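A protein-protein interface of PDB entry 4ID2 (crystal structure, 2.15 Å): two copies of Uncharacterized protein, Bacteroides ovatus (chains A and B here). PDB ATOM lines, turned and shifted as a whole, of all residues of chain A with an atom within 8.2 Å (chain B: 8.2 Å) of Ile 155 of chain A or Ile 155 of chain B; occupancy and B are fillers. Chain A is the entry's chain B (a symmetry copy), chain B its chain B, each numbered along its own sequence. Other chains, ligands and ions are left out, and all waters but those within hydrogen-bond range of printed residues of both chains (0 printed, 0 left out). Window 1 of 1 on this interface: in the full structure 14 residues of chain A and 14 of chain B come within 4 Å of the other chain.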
ATOM      1  N   PHE A 102      -2.266  13.065   0.716  1.00  0.00           N
ATOM      2  CA  PHE A 102      -1.329  14.049   0.165  1.00  0.00           C
ATOM      3  C   PHE A 102      -1.925  14.750  -1.069  1.00  0.00           C
ATOM      4  O   PHE A 102      -1.680  15.938  -1.247  1.00  0.00           O
ATOM      5  CB  PHE A 102       0.024  13.407  -0.188  1.00  0.00           C
ATOM      6  CG  PHE A 102       0.974  14.366  -0.870  1.00  0.00           C
ATOM      7  CD1 PHE A 102       1.545  15.417  -0.169  1.00  0.00           C
ATOM      8  CD2 PHE A 102       1.179  14.305  -2.242  1.00  0.00           C
ATOM      9  CE1 PHE A 102       2.340  16.362  -0.822  1.00  0.00           C
ATOM     10  CE2 PHE A 102       1.984  15.238  -2.887  1.00  0.00           C
ATOM     11  CZ  PHE A 102       2.581  16.249  -2.170  1.00  0.00           C
ATOM     12  N   LEU A 134       7.799  22.680  -1.594  1.00  0.00           N
ATOM     13  CA  LEU A 134       7.718  21.220  -1.549  1.00  0.00           C
ATOM     14  C   LEU A 134       6.807  20.657  -2.630  1.00  0.00           C
ATOM     15  O   LEU A 134       5.667  21.100  -2.763  1.00  0.00           O
ATOM     16  CB  LEU A 134       7.206  20.759  -0.180  1.00  0.00           C
ATOM     17  CG  LEU A 134       8.102  21.126   0.995  1.00  0.00           C
ATOM     18  CD1 LEU A 134       7.319  21.187   2.262  1.00  0.00           C
ATOM     19  CD2 LEU A 134       9.230  20.137   1.143  1.00  0.00           C
ATOM     20  N   TYR A 135       7.284  19.638  -3.356  1.00  0.00           N
ATOM     21  CA  TYR A 135       6.512  19.012  -4.417  1.00  0.00           C
ATOM     22  C   TYR A 135       6.820  17.530  -4.559  1.00  0.00           C
ATOM     23  O   TYR A 135       7.885  17.058  -4.174  1.00  0.00           O
ATOM     24  CB  TYR A 135       6.783  19.720  -5.766  1.00  0.00           C
ATOM     25  CG  TYR A 135       8.184  19.488  -6.296  1.00  0.00           C
ATOM     26  CD1 TYR A 135       9.237  20.311  -5.919  1.00  0.00           C
ATOM     27  CD2 TYR A 135       8.466  18.408  -7.124  1.00  0.00           C
ATOM     28  CE1 TYR A 135      10.541  20.061  -6.343  1.00  0.00           C
ATOM     29  CE2 TYR A 135       9.764  18.144  -7.554  1.00  0.00           C
ATOM     30  CZ  TYR A 135      10.801  18.980  -7.172  1.00  0.00           C
ATOM     31  OH  TYR A 135      12.094  18.735  -7.577  1.00  0.00           O
ATOM     32  N   MET A 136       5.902  16.824  -5.193  1.00  0.00           N
ATOM     33  CA  MET A 136       6.026  15.410  -5.495  1.00  0.00           C
ATOM     34  C   MET A 136       6.220  15.219  -6.998  1.00  0.00           C
ATOM     35  O   MET A 136       5.348  15.604  -7.771  1.00  0.00           O
ATOM     36  CB  MET A 136       4.775  14.689  -5.036  1.00  0.00           C
ATOM     37  CG  MET A 136       4.793  13.202  -5.330  1.00  0.00           C
ATOM     38  SD  MET A 136       3.186  12.401  -4.685  1.00  0.00           S
ATOM     39  CE  MET A 136       3.766  11.947  -2.916  1.00  0.00           C
ATOM     40  N   PRO A 137       7.331  14.585  -7.425  1.00  0.00           N
ATOM     41  CA  PRO A 137       7.539  14.364  -8.862  1.00  0.00           C
ATOM     42  C   PRO A 137       6.669  13.230  -9.403  1.00  0.00           C
ATOM     43  O   PRO A 137       6.542  12.182  -8.764  1.00  0.00           O
ATOM     44  CB  PRO A 137       9.031  14.028  -8.950  1.00  0.00           C
ATOM     45  CG  PRO A 137       9.359  13.441  -7.641  1.00  0.00           C
ATOM     46  CD  PRO A 137       8.459  14.070  -6.628  1.00  0.00           C
ATOM     47  N   LEU A 138       6.043  13.469 -10.572  1.00  0.00           N
ATOM     48  CA  LEU A 138       5.171  12.523 -11.275  1.00  0.00           C
ATOM     49  C   LEU A 138       5.549  12.523 -12.757  1.00  0.00           C
ATOM     50  O   LEU A 138       6.305  13.398 -13.180  1.00  0.00           O
ATOM     51  CB  LEU A 138       3.691  12.945 -11.102  1.00  0.00           C
ATOM     52  CG  LEU A 138       3.224  13.207  -9.664  1.00  0.00           C
ATOM     53  CD1 LEU A 138       2.052  14.169  -9.623  1.00  0.00           C
ATOM     54  CD2 LEU A 138       2.906  11.910  -8.956  1.00  0.00           C
ATOM     55  N   LYS A 152       4.027   7.497 -11.024  1.00  0.00           N
ATOM     56  CA  LYS A 152       4.595   8.279  -9.918  1.00  0.00           C
ATOM     57  C   LYS A 152       6.082   7.982  -9.907  1.00  0.00           C
ATOM     58  O   LYS A 152       6.476   6.844 -10.156  1.00  0.00           O
ATOM     59  CB  LYS A 152       3.940   7.910  -8.570  1.00  0.00           C
ATOM     60  CG  LYS A 152       4.325   8.803  -7.388  1.00  0.00           C
ATOM     61  CD  LYS A 152       4.252   8.046  -6.055  1.00  0.00           C
ATOM     62  CE  LYS A 152       3.883   8.942  -4.899  1.00  0.00           C
ATOM     63  NZ  LYS A 152       3.775   8.196  -3.617  1.00  0.00           N
ATOM     64  N   VAL A 153       6.909   8.994  -9.659  1.00  0.00           N
ATOM     65  CA  VAL A 153       8.352   8.803  -9.598  1.00  0.00           C
ATOM     66  C   VAL A 153       8.667   8.264  -8.198  1.00  0.00           C
ATOM     67  O   VAL A 153       8.247   8.870  -7.209  1.00  0.00           O
ATOM     68  CB  VAL A 153       9.096  10.119  -9.925  1.00  0.00           C
ATOM     69  CG1 VAL A 153      10.607   9.953  -9.781  1.00  0.00           C
ATOM     70  CG2 VAL A 153       8.731  10.616 -11.328  1.00  0.00           C
ATOM     71  N   ASP A 154       9.352   7.108  -8.113  1.00  0.00           N
ATOM     72  CA  ASP A 154       9.707   6.506  -6.825  1.00  0.00           C
ATOM     73  C   ASP A 154      10.998   7.124  -6.326  1.00  0.00           C
ATOM     74  O   ASP A 154      12.009   7.073  -7.031  1.00  0.00           O
ATOM     75  CB  ASP A 154       9.848   4.973  -6.929  1.00  0.00           C
ATOM     76  CG  ASP A 154       8.554   4.194  -6.783  1.00  0.00           C
ATOM     77  OD1 ASP A 154       7.469   4.810  -6.887  1.00  0.00           O
ATOM     78  OD2 ASP A 154       8.626   2.969  -6.563  1.00  0.00           O
ATOM     79  N   ILE A 155      10.983   7.693  -5.117  1.00  0.00           N
ATOM     80  CA  ILE A 155      12.159   8.331  -4.548  1.00  0.00           C
ATOM     81  C   ILE A 155      12.796   7.352  -3.589  1.00  0.00           C
ATOM     82  O   ILE A 155      12.119   6.883  -2.683  1.00  0.00           O
ATOM     83  CB  ILE A 155      11.781   9.672  -3.868  1.00  0.00           C
ATOM     84  CG1 ILE A 155      10.936  10.555  -4.832  1.00  0.00           C
ATOM     85  CG2 ILE A 155      13.048  10.405  -3.406  1.00  0.00           C
ATOM     86  CD1 ILE A 155      10.545  11.897  -4.299  1.00  0.00           C
ATOM     87  N   LEU A 156      14.094   7.053  -3.770  1.00  0.00           N
ATOM     88  CA  LEU A 156      14.805   6.134  -2.890  1.00  0.00           C
ATOM     89  C   LEU A 156      15.784   6.946  -2.087  1.00  0.00           C
ATOM     90  O   LEU A 156      16.249   7.975  -2.564  1.00  0.00           O
ATOM     91  CB  LEU A 156      15.535   5.031  -3.663  1.00  0.00           C
ATOM     92  CG  LEU A 156      14.711   4.147  -4.596  1.00  0.00           C
ATOM     93  CD1 LEU A 156      15.551   2.982  -5.077  1.00  0.00           C
ATOM     94  CD2 LEU A 156      13.477   3.591  -3.912  1.00  0.00           C
ATOM     95  N   GLU A 157      16.092   6.500  -0.875  1.00  0.00           N
ATOM     96  CA  GLU A 157      17.012   7.188   0.021  1.00  0.00           C
ATOM     97  C   GLU A 157      18.300   6.428   0.154  1.00  0.00           C
ATOM     98  O   GLU A 157      18.262   5.204   0.230  1.00  0.00           O
ATOM     99  CB  GLU A 157      16.377   7.352   1.402  1.00  0.00           C
ATOM    100  CG  GLU A 157      15.261   8.376   1.419  1.00  0.00           C
ATOM    101  CD  GLU A 157      14.576   8.552   2.754  1.00  0.00           C
ATOM    102  OE1 GLU A 157      14.902   7.821   3.716  1.00  0.00           O
ATOM    103  OE2 GLU A 157      13.691   9.432   2.830  1.00  0.00           O
ATOM    104  N   GLU A 158      19.438   7.153   0.260  1.00  0.00           N
ATOM    105  CA  GLU A 158      20.761   6.562   0.455  1.00  0.00           C
ATOM    106  C   GLU A 158      21.340   7.052   1.787  1.00  0.00           C
ATOM    107  O   GLU A 158      21.243   8.240   2.098  1.00  0.00           O
ATOM    108  CB  GLU A 158      21.707   6.863  -0.725  1.00  0.00           C
ATOM    109  CG  GLU A 158      21.996   8.330  -0.999  1.00  0.00           C
ATOM    110  CD  GLU A 158      23.056   8.530  -2.062  1.00  0.00           C
ATOM    111  OE1 GLU A 158      22.883   7.989  -3.177  1.00  0.00           O
ATOM    112  OE2 GLU A 158      24.066   9.214  -1.777  1.00  0.00           O
ATOM    113  N   PHE B 102       8.871  -1.935  -7.981  1.00  0.00           N
ATOM    114  CA  PHE B 102       9.944  -1.665  -7.021  1.00  0.00           C
ATOM    115  C   PHE B 102       9.968  -2.723  -5.903  1.00  0.00           C
ATOM    116  O   PHE B 102      11.051  -3.082  -5.454  1.00  0.00           O
ATOM    117  CB  PHE B 102       9.822  -0.255  -6.416  1.00  0.00           C
ATOM    118  CG  PHE B 102      10.841   0.016  -5.333  1.00  0.00           C
ATOM    119  CD1 PHE B 102      12.185   0.160  -5.643  1.00  0.00           C
ATOM    120  CD2 PHE B 102      10.479  -0.022  -3.993  1.00  0.00           C
ATOM    121  CE1 PHE B 102      13.139   0.307  -4.634  1.00  0.00           C
ATOM    122  CE2 PHE B 102      11.429   0.141  -2.990  1.00  0.00           C
ATOM    123  CZ  PHE B 102      12.752   0.329  -3.315  1.00  0.00           C
ATOM    124  N   LEU B 134      20.600   2.054  -1.228  1.00  0.00           N
ATOM    125  CA  LEU B 134      19.307   2.656  -1.553  1.00  0.00           C
ATOM    126  C   LEU B 134      18.146   1.926  -0.895  1.00  0.00           C
ATOM    127  O   LEU B 134      18.041   0.705  -1.015  1.00  0.00           O
ATOM    128  CB  LEU B 134      19.091   2.663  -3.070  1.00  0.00           C
ATOM    129  CG  LEU B 134      20.103   3.486  -3.857  1.00  0.00           C
ATOM    130  CD1 LEU B 134      20.206   3.000  -5.262  1.00  0.00           C
ATOM    131  CD2 LEU B 134      19.729   4.947  -3.851  1.00  0.00           C
ATOM    132  N   TYR B 135      17.239   2.677  -0.256  1.00  0.00           N
ATOM    133  CA  TYR B 135      16.084   2.100   0.412  1.00  0.00           C
ATOM    134  C   TYR B 135      14.874   3.018   0.370  1.00  0.00           C
ATOM    135  O   TYR B 135      14.995   4.231   0.227  1.00  0.00           O
ATOM    136  CB  TYR B 135      16.426   1.773   1.886  1.00  0.00           C
ATOM    137  CG  TYR B 135      16.629   3.008   2.743  1.00  0.00           C
ATOM    138  CD1 TYR B 135      17.873   3.618   2.834  1.00  0.00           C
ATOM    139  CD2 TYR B 135      15.563   3.598   3.411  1.00  0.00           C
ATOM    140  CE1 TYR B 135      18.052   4.794   3.561  1.00  0.00           C
ATOM    141  CE2 TYR B 135      15.726   4.774   4.139  1.00  0.00           C
ATOM    142  CZ  TYR B 135      16.976   5.366   4.223  1.00  0.00           C
ATOM    143  OH  TYR B 135      17.161   6.533   4.930  1.00  0.00           O
ATOM    144  N   MET B 136      13.712   2.426   0.580  1.00  0.00           N
ATOM    145  CA  MET B 136      12.442   3.125   0.648  1.00  0.00           C
ATOM    146  C   MET B 136      11.924   3.114   2.085  1.00  0.00           C
ATOM    147  O   MET B 136      11.693   2.040   2.633  1.00  0.00           O
ATOM    148  CB  MET B 136      11.447   2.444  -0.268  1.00  0.00           C
ATOM    149  CG  MET B 136      10.073   3.084  -0.250  1.00  0.00           C
ATOM    150  SD  MET B 136       8.919   2.162  -1.458  1.00  0.00           S
ATOM    151  CE  MET B 136       9.258   3.189  -3.041  1.00  0.00           C
ATOM    152  N   PRO B 137      11.691   4.296   2.692  1.00  0.00           N
ATOM    153  CA  PRO B 137      11.172   4.323   4.065  1.00  0.00           C
ATOM    154  C   PRO B 137       9.683   3.984   4.125  1.00  0.00           C
ATOM    155  O   PRO B 137       8.900   4.464   3.301  1.00  0.00           O
ATOM    156  CB  PRO B 137      11.447   5.761   4.513  1.00  0.00           C
ATOM    157  CG  PRO B 137      11.438   6.548   3.269  1.00  0.00           C
ATOM    158  CD  PRO B 137      11.917   5.656   2.171  1.00  0.00           C
ATOM    159  N   LEU B 138       9.309   3.121   5.091  1.00  0.00           N
ATOM    160  CA  LEU B 138       7.938   2.667   5.336  1.00  0.00           C
ATOM    161  C   LEU B 138       7.665   2.732   6.840  1.00  0.00           C
ATOM    162  O   LEU B 138       8.609   2.918   7.609  1.00  0.00           O
ATOM    163  CB  LEU B 138       7.767   1.213   4.826  1.00  0.00           C
ATOM    164  CG  LEU B 138       8.219   0.943   3.386  1.00  0.00           C
ATOM    165  CD1 LEU B 138       8.604  -0.511   3.184  1.00  0.00           C
ATOM    166  CD2 LEU B 138       7.163   1.382   2.398  1.00  0.00           C
ATOM    167  N   LYS B 152       3.170   4.002   3.880  1.00  0.00           N
ATOM    168  CA  LYS B 152       4.393   4.338   3.139  1.00  0.00           C
ATOM    169  C   LYS B 152       4.728   5.772   3.500  1.00  0.00           C
ATOM    170  O   LYS B 152       3.821   6.590   3.644  1.00  0.00           O
ATOM    171  CB  LYS B 152       4.195   4.174   1.617  1.00  0.00           C
ATOM    172  CG  LYS B 152       5.463   4.314   0.772  1.00  0.00           C
ATOM    173  CD  LYS B 152       5.154   4.832  -0.639  1.00  0.00           C
ATOM    174  CE  LYS B 152       6.118   4.308  -1.673  1.00  0.00           C
ATOM    175  NZ  LYS B 152       5.790   4.781  -3.044  1.00  0.00           N
ATOM    176  N   VAL B 153       6.010   6.077   3.681  1.00  0.00           N
ATOM    177  CA  VAL B 153       6.434   7.434   4.001  1.00  0.00           C
ATOM    178  C   VAL B 153       6.488   8.203   2.677  1.00  0.00           C
ATOM    179  O   VAL B 153       7.132   7.736   1.733  1.00  0.00           O
ATOM    180  CB  VAL B 153       7.785   7.425   4.755  1.00  0.00           C
ATOM    181  CG1 VAL B 153       8.282   8.844   5.020  1.00  0.00           C
ATOM    182  CG2 VAL B 153       7.673   6.631   6.061  1.00  0.00           C
ATOM    183  N   ASP B 154       5.777   9.342   2.585  1.00  0.00           N
ATOM    184  CA  ASP B 154       5.759  10.155   1.367  1.00  0.00           C
ATOM    185  C   ASP B 154       6.954  11.089   1.375  1.00  0.00           C
ATOM    186  O   ASP B 154       7.110  11.868   2.317  1.00  0.00           O
ATOM    187  CB  ASP B 154       4.449  10.958   1.232  1.00  0.00           C
ATOM    188  CG  ASP B 154       3.296  10.210   0.588  1.00  0.00           C
ATOM    189  OD1 ASP B 154       3.373   8.964   0.486  1.00  0.00           O
ATOM    190  OD2 ASP B 154       2.319  10.870   0.183  1.00  0.00           O
ATOM    191  N   ILE B 155       7.789  11.031   0.332  1.00  0.00           N
ATOM    192  CA  ILE B 155       8.974  11.868   0.245  1.00  0.00           C
ATOM    193  C   ILE B 155       8.647  13.039  -0.651  1.00  0.00           C
ATOM    194  O   ILE B 155       8.227  12.824  -1.781  1.00  0.00           O
ATOM    195  CB  ILE B 155      10.188  11.048  -0.265  1.00  0.00           C
ATOM    196  CG1 ILE B 155      10.347   9.738   0.560  1.00  0.00           C
ATOM    197  CG2 ILE B 155      11.462  11.901  -0.208  1.00  0.00           C
ATOM    198  CD1 ILE B 155      11.515   8.879   0.185  1.00  0.00           C
ATOM    199  N   LEU B 156       8.850  14.276  -0.164  1.00  0.00           N
ATOM    200  CA  LEU B 156       8.582  15.471  -0.954  1.00  0.00           C
ATOM    201  C   LEU B 156       9.908  16.098  -1.287  1.00  0.00           C
ATOM    202  O   LEU B 156      10.854  15.950  -0.522  1.00  0.00           O
ATOM    203  CB  LEU B 156       7.689  16.473  -0.214  1.00  0.00           C
ATOM    204  CG  LEU B 156       6.325  15.991   0.273  1.00  0.00           C
ATOM    205  CD1 LEU B 156       5.506  17.168   0.758  1.00  0.00           C
ATOM    206  CD2 LEU B 156       5.545  15.289  -0.822  1.00  0.00           C
ATOM    207  N   GLU B 157       9.986  16.786  -2.420  1.00  0.00           N
ATOM    208  CA  GLU B 157      11.208  17.434  -2.879  1.00  0.00           C
ATOM    209  C   GLU B 157      11.095  18.928  -2.773  1.00  0.00           C
ATOM    210  O   GLU B 157      10.033  19.465  -3.073  1.00  0.00           O
ATOM    211  CB  GLU B 157      11.492  17.051  -4.332  1.00  0.00           C
ATOM    212  CG  GLU B 157      11.946  15.614  -4.484  1.00  0.00           C
ATOM    213  CD  GLU B 157      12.208  15.173  -5.906  1.00  0.00           C
ATOM    214  OE1 GLU B 157      11.974  15.962  -6.849  1.00  0.00           O
ATOM    215  OE2 GLU B 157      12.645  14.014  -6.072  1.00  0.00           O
ATOM    216  N   GLU B 158      12.210  19.608  -2.420  1.00  0.00           N
ATOM    217  CA  GLU B 158      12.275  21.066  -2.332  1.00  0.00           C
ATOM    218  C   GLU B 158      13.312  21.585  -3.334  1.00  0.00           C
ATOM    219  O   GLU B 158      14.398  21.014  -3.444  1.00  0.00           O
ATOM    220  CB  GLU B 158      12.578  21.545  -0.897  1.00  0.00           C
ATOM    221  CG  GLU B 158      13.894  21.080  -0.296  1.00  0.00           C
ATOM    222  CD  GLU B 158      14.187  21.724   1.043  1.00  0.00           C
ATOM    223  OE1 GLU B 158      13.328  21.621   1.948  1.00  0.00           O
ATOM    224  OE2 GLU B 158      15.267  22.344   1.184  1.00  0.00           O
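The backbone carbonyl oxygen (O) of Tyr 135 of chain A sits at hydrogen-bond distance from the backbone NH (N) of Glu 157 of chain B, 2.8 Å away. The backbone carbonyl oxygen (O) of Tyr 135 of chain B sits at hydrogen-bond distance from the backbone NH (N) of Glu 157 of chain A (2.8 Å).
N of Val 153 of chain B lies within hydrogen-bond range of O of Pro 137 of chain B, 3.3 Å away. O of Pro 137 of chain A lies within hydrogen-bond range of N of Val 153 of chain A (3.3 Å).
Among the printed residues, pairs that only touch across the chains: Phe 102 of chain A with Asp 154 of chain B, Phe 102 of chain A with Leu 156 of chain B, Leu 134 of chain A with Glu 157 of chain B, Tyr 135 of chain A with Leu 156 of chain B, Met 136 of chain A with Asp 154 of chain B, Pro 137 of chain A with Glu 157 of chain B, Asp 154 of chain A with Phe 102 of chain B, Asp 154 of chain A with Met 136 of chain B, Ile 155 of chain A with Ile 155 of chain B, Ile 155 of chain A with Glu 157 of chain B, Leu 156 of chain A with Phe 102 of chain B, Leu 156 of chain A with Tyr 135 of chain B, Glu 157 of chain A with Leu 134 of chain B, Glu 157 of chain A with Pro 137 of chain B and Glu 157 of chain A with Ile 155 of chain B.
Of chain B, only Ile 155 and Glu 157 come within 4 Å of Ile 155 of chain A. Printed residues of chain B within 4 Å of Leu 156 of chain A: Phe 102 (3.4 Å) and Tyr 135 (3.7 Å). Of the printed residues of chain A, Leu 134 of chain B touches Glu 157. Of the printed residues of chain A, Asp 154 of chain B touches Phe 102 and Met 136. Ile 155 of chain B touches two residues of chain A. Of the printed residues of chain A, Leu 156 of chain B touches Phe 102 and Tyr 135. Of the printed residues of chain A, Glu 157 of chain B touches Leu 134, Tyr 135, Pro 137 and Ile 155. The nearest residue of chain B that does not touch Ile 155 of chain A is Met 136 of chain B (4.7 Å). The nearest residue of chain A that does not touch Ile 155 of chain B is Met 136 of chain A (4.7 Å).
Along chain A the printed residues that touch a printed residue of chain B span positions 102 to 157. Of the 13 printed residues of chain B, 9 touch a printed residue of chain A. Along chain B the printed residues that touch a printed residue of chain A span positions 102 to 157. Among the printed residues, 17 pairs touch across the chains.
Phe 102 of chain A touches Asp 154 of chain B, and with the chains exchanged Asp 154 of chain A touches Phe 102 of chain B. Leu 134 of chain A touches Glu 157 of chain B, and with the chains exchanged Glu 157 of chain A touches Leu 134 of chain B. Tyr 135 of chain A touches Leu 156 of chain B, and with the chains exchanged Leu 156 of chain A touches Tyr 135 of chain B. Ile 155 of chain A touches Glu 157 of chain B, and with the chains exchanged Glu 157 of chain A touches Ile 155 of chain B. Positions printed for both chains: 102, 134, 135, 136, 137, 138, 152, 153, 154, 155, 156, 157 and 158. Of the 17 pairs that touch across the chains among the printed residues, 17 have their exchanged pair printed and touching as well.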
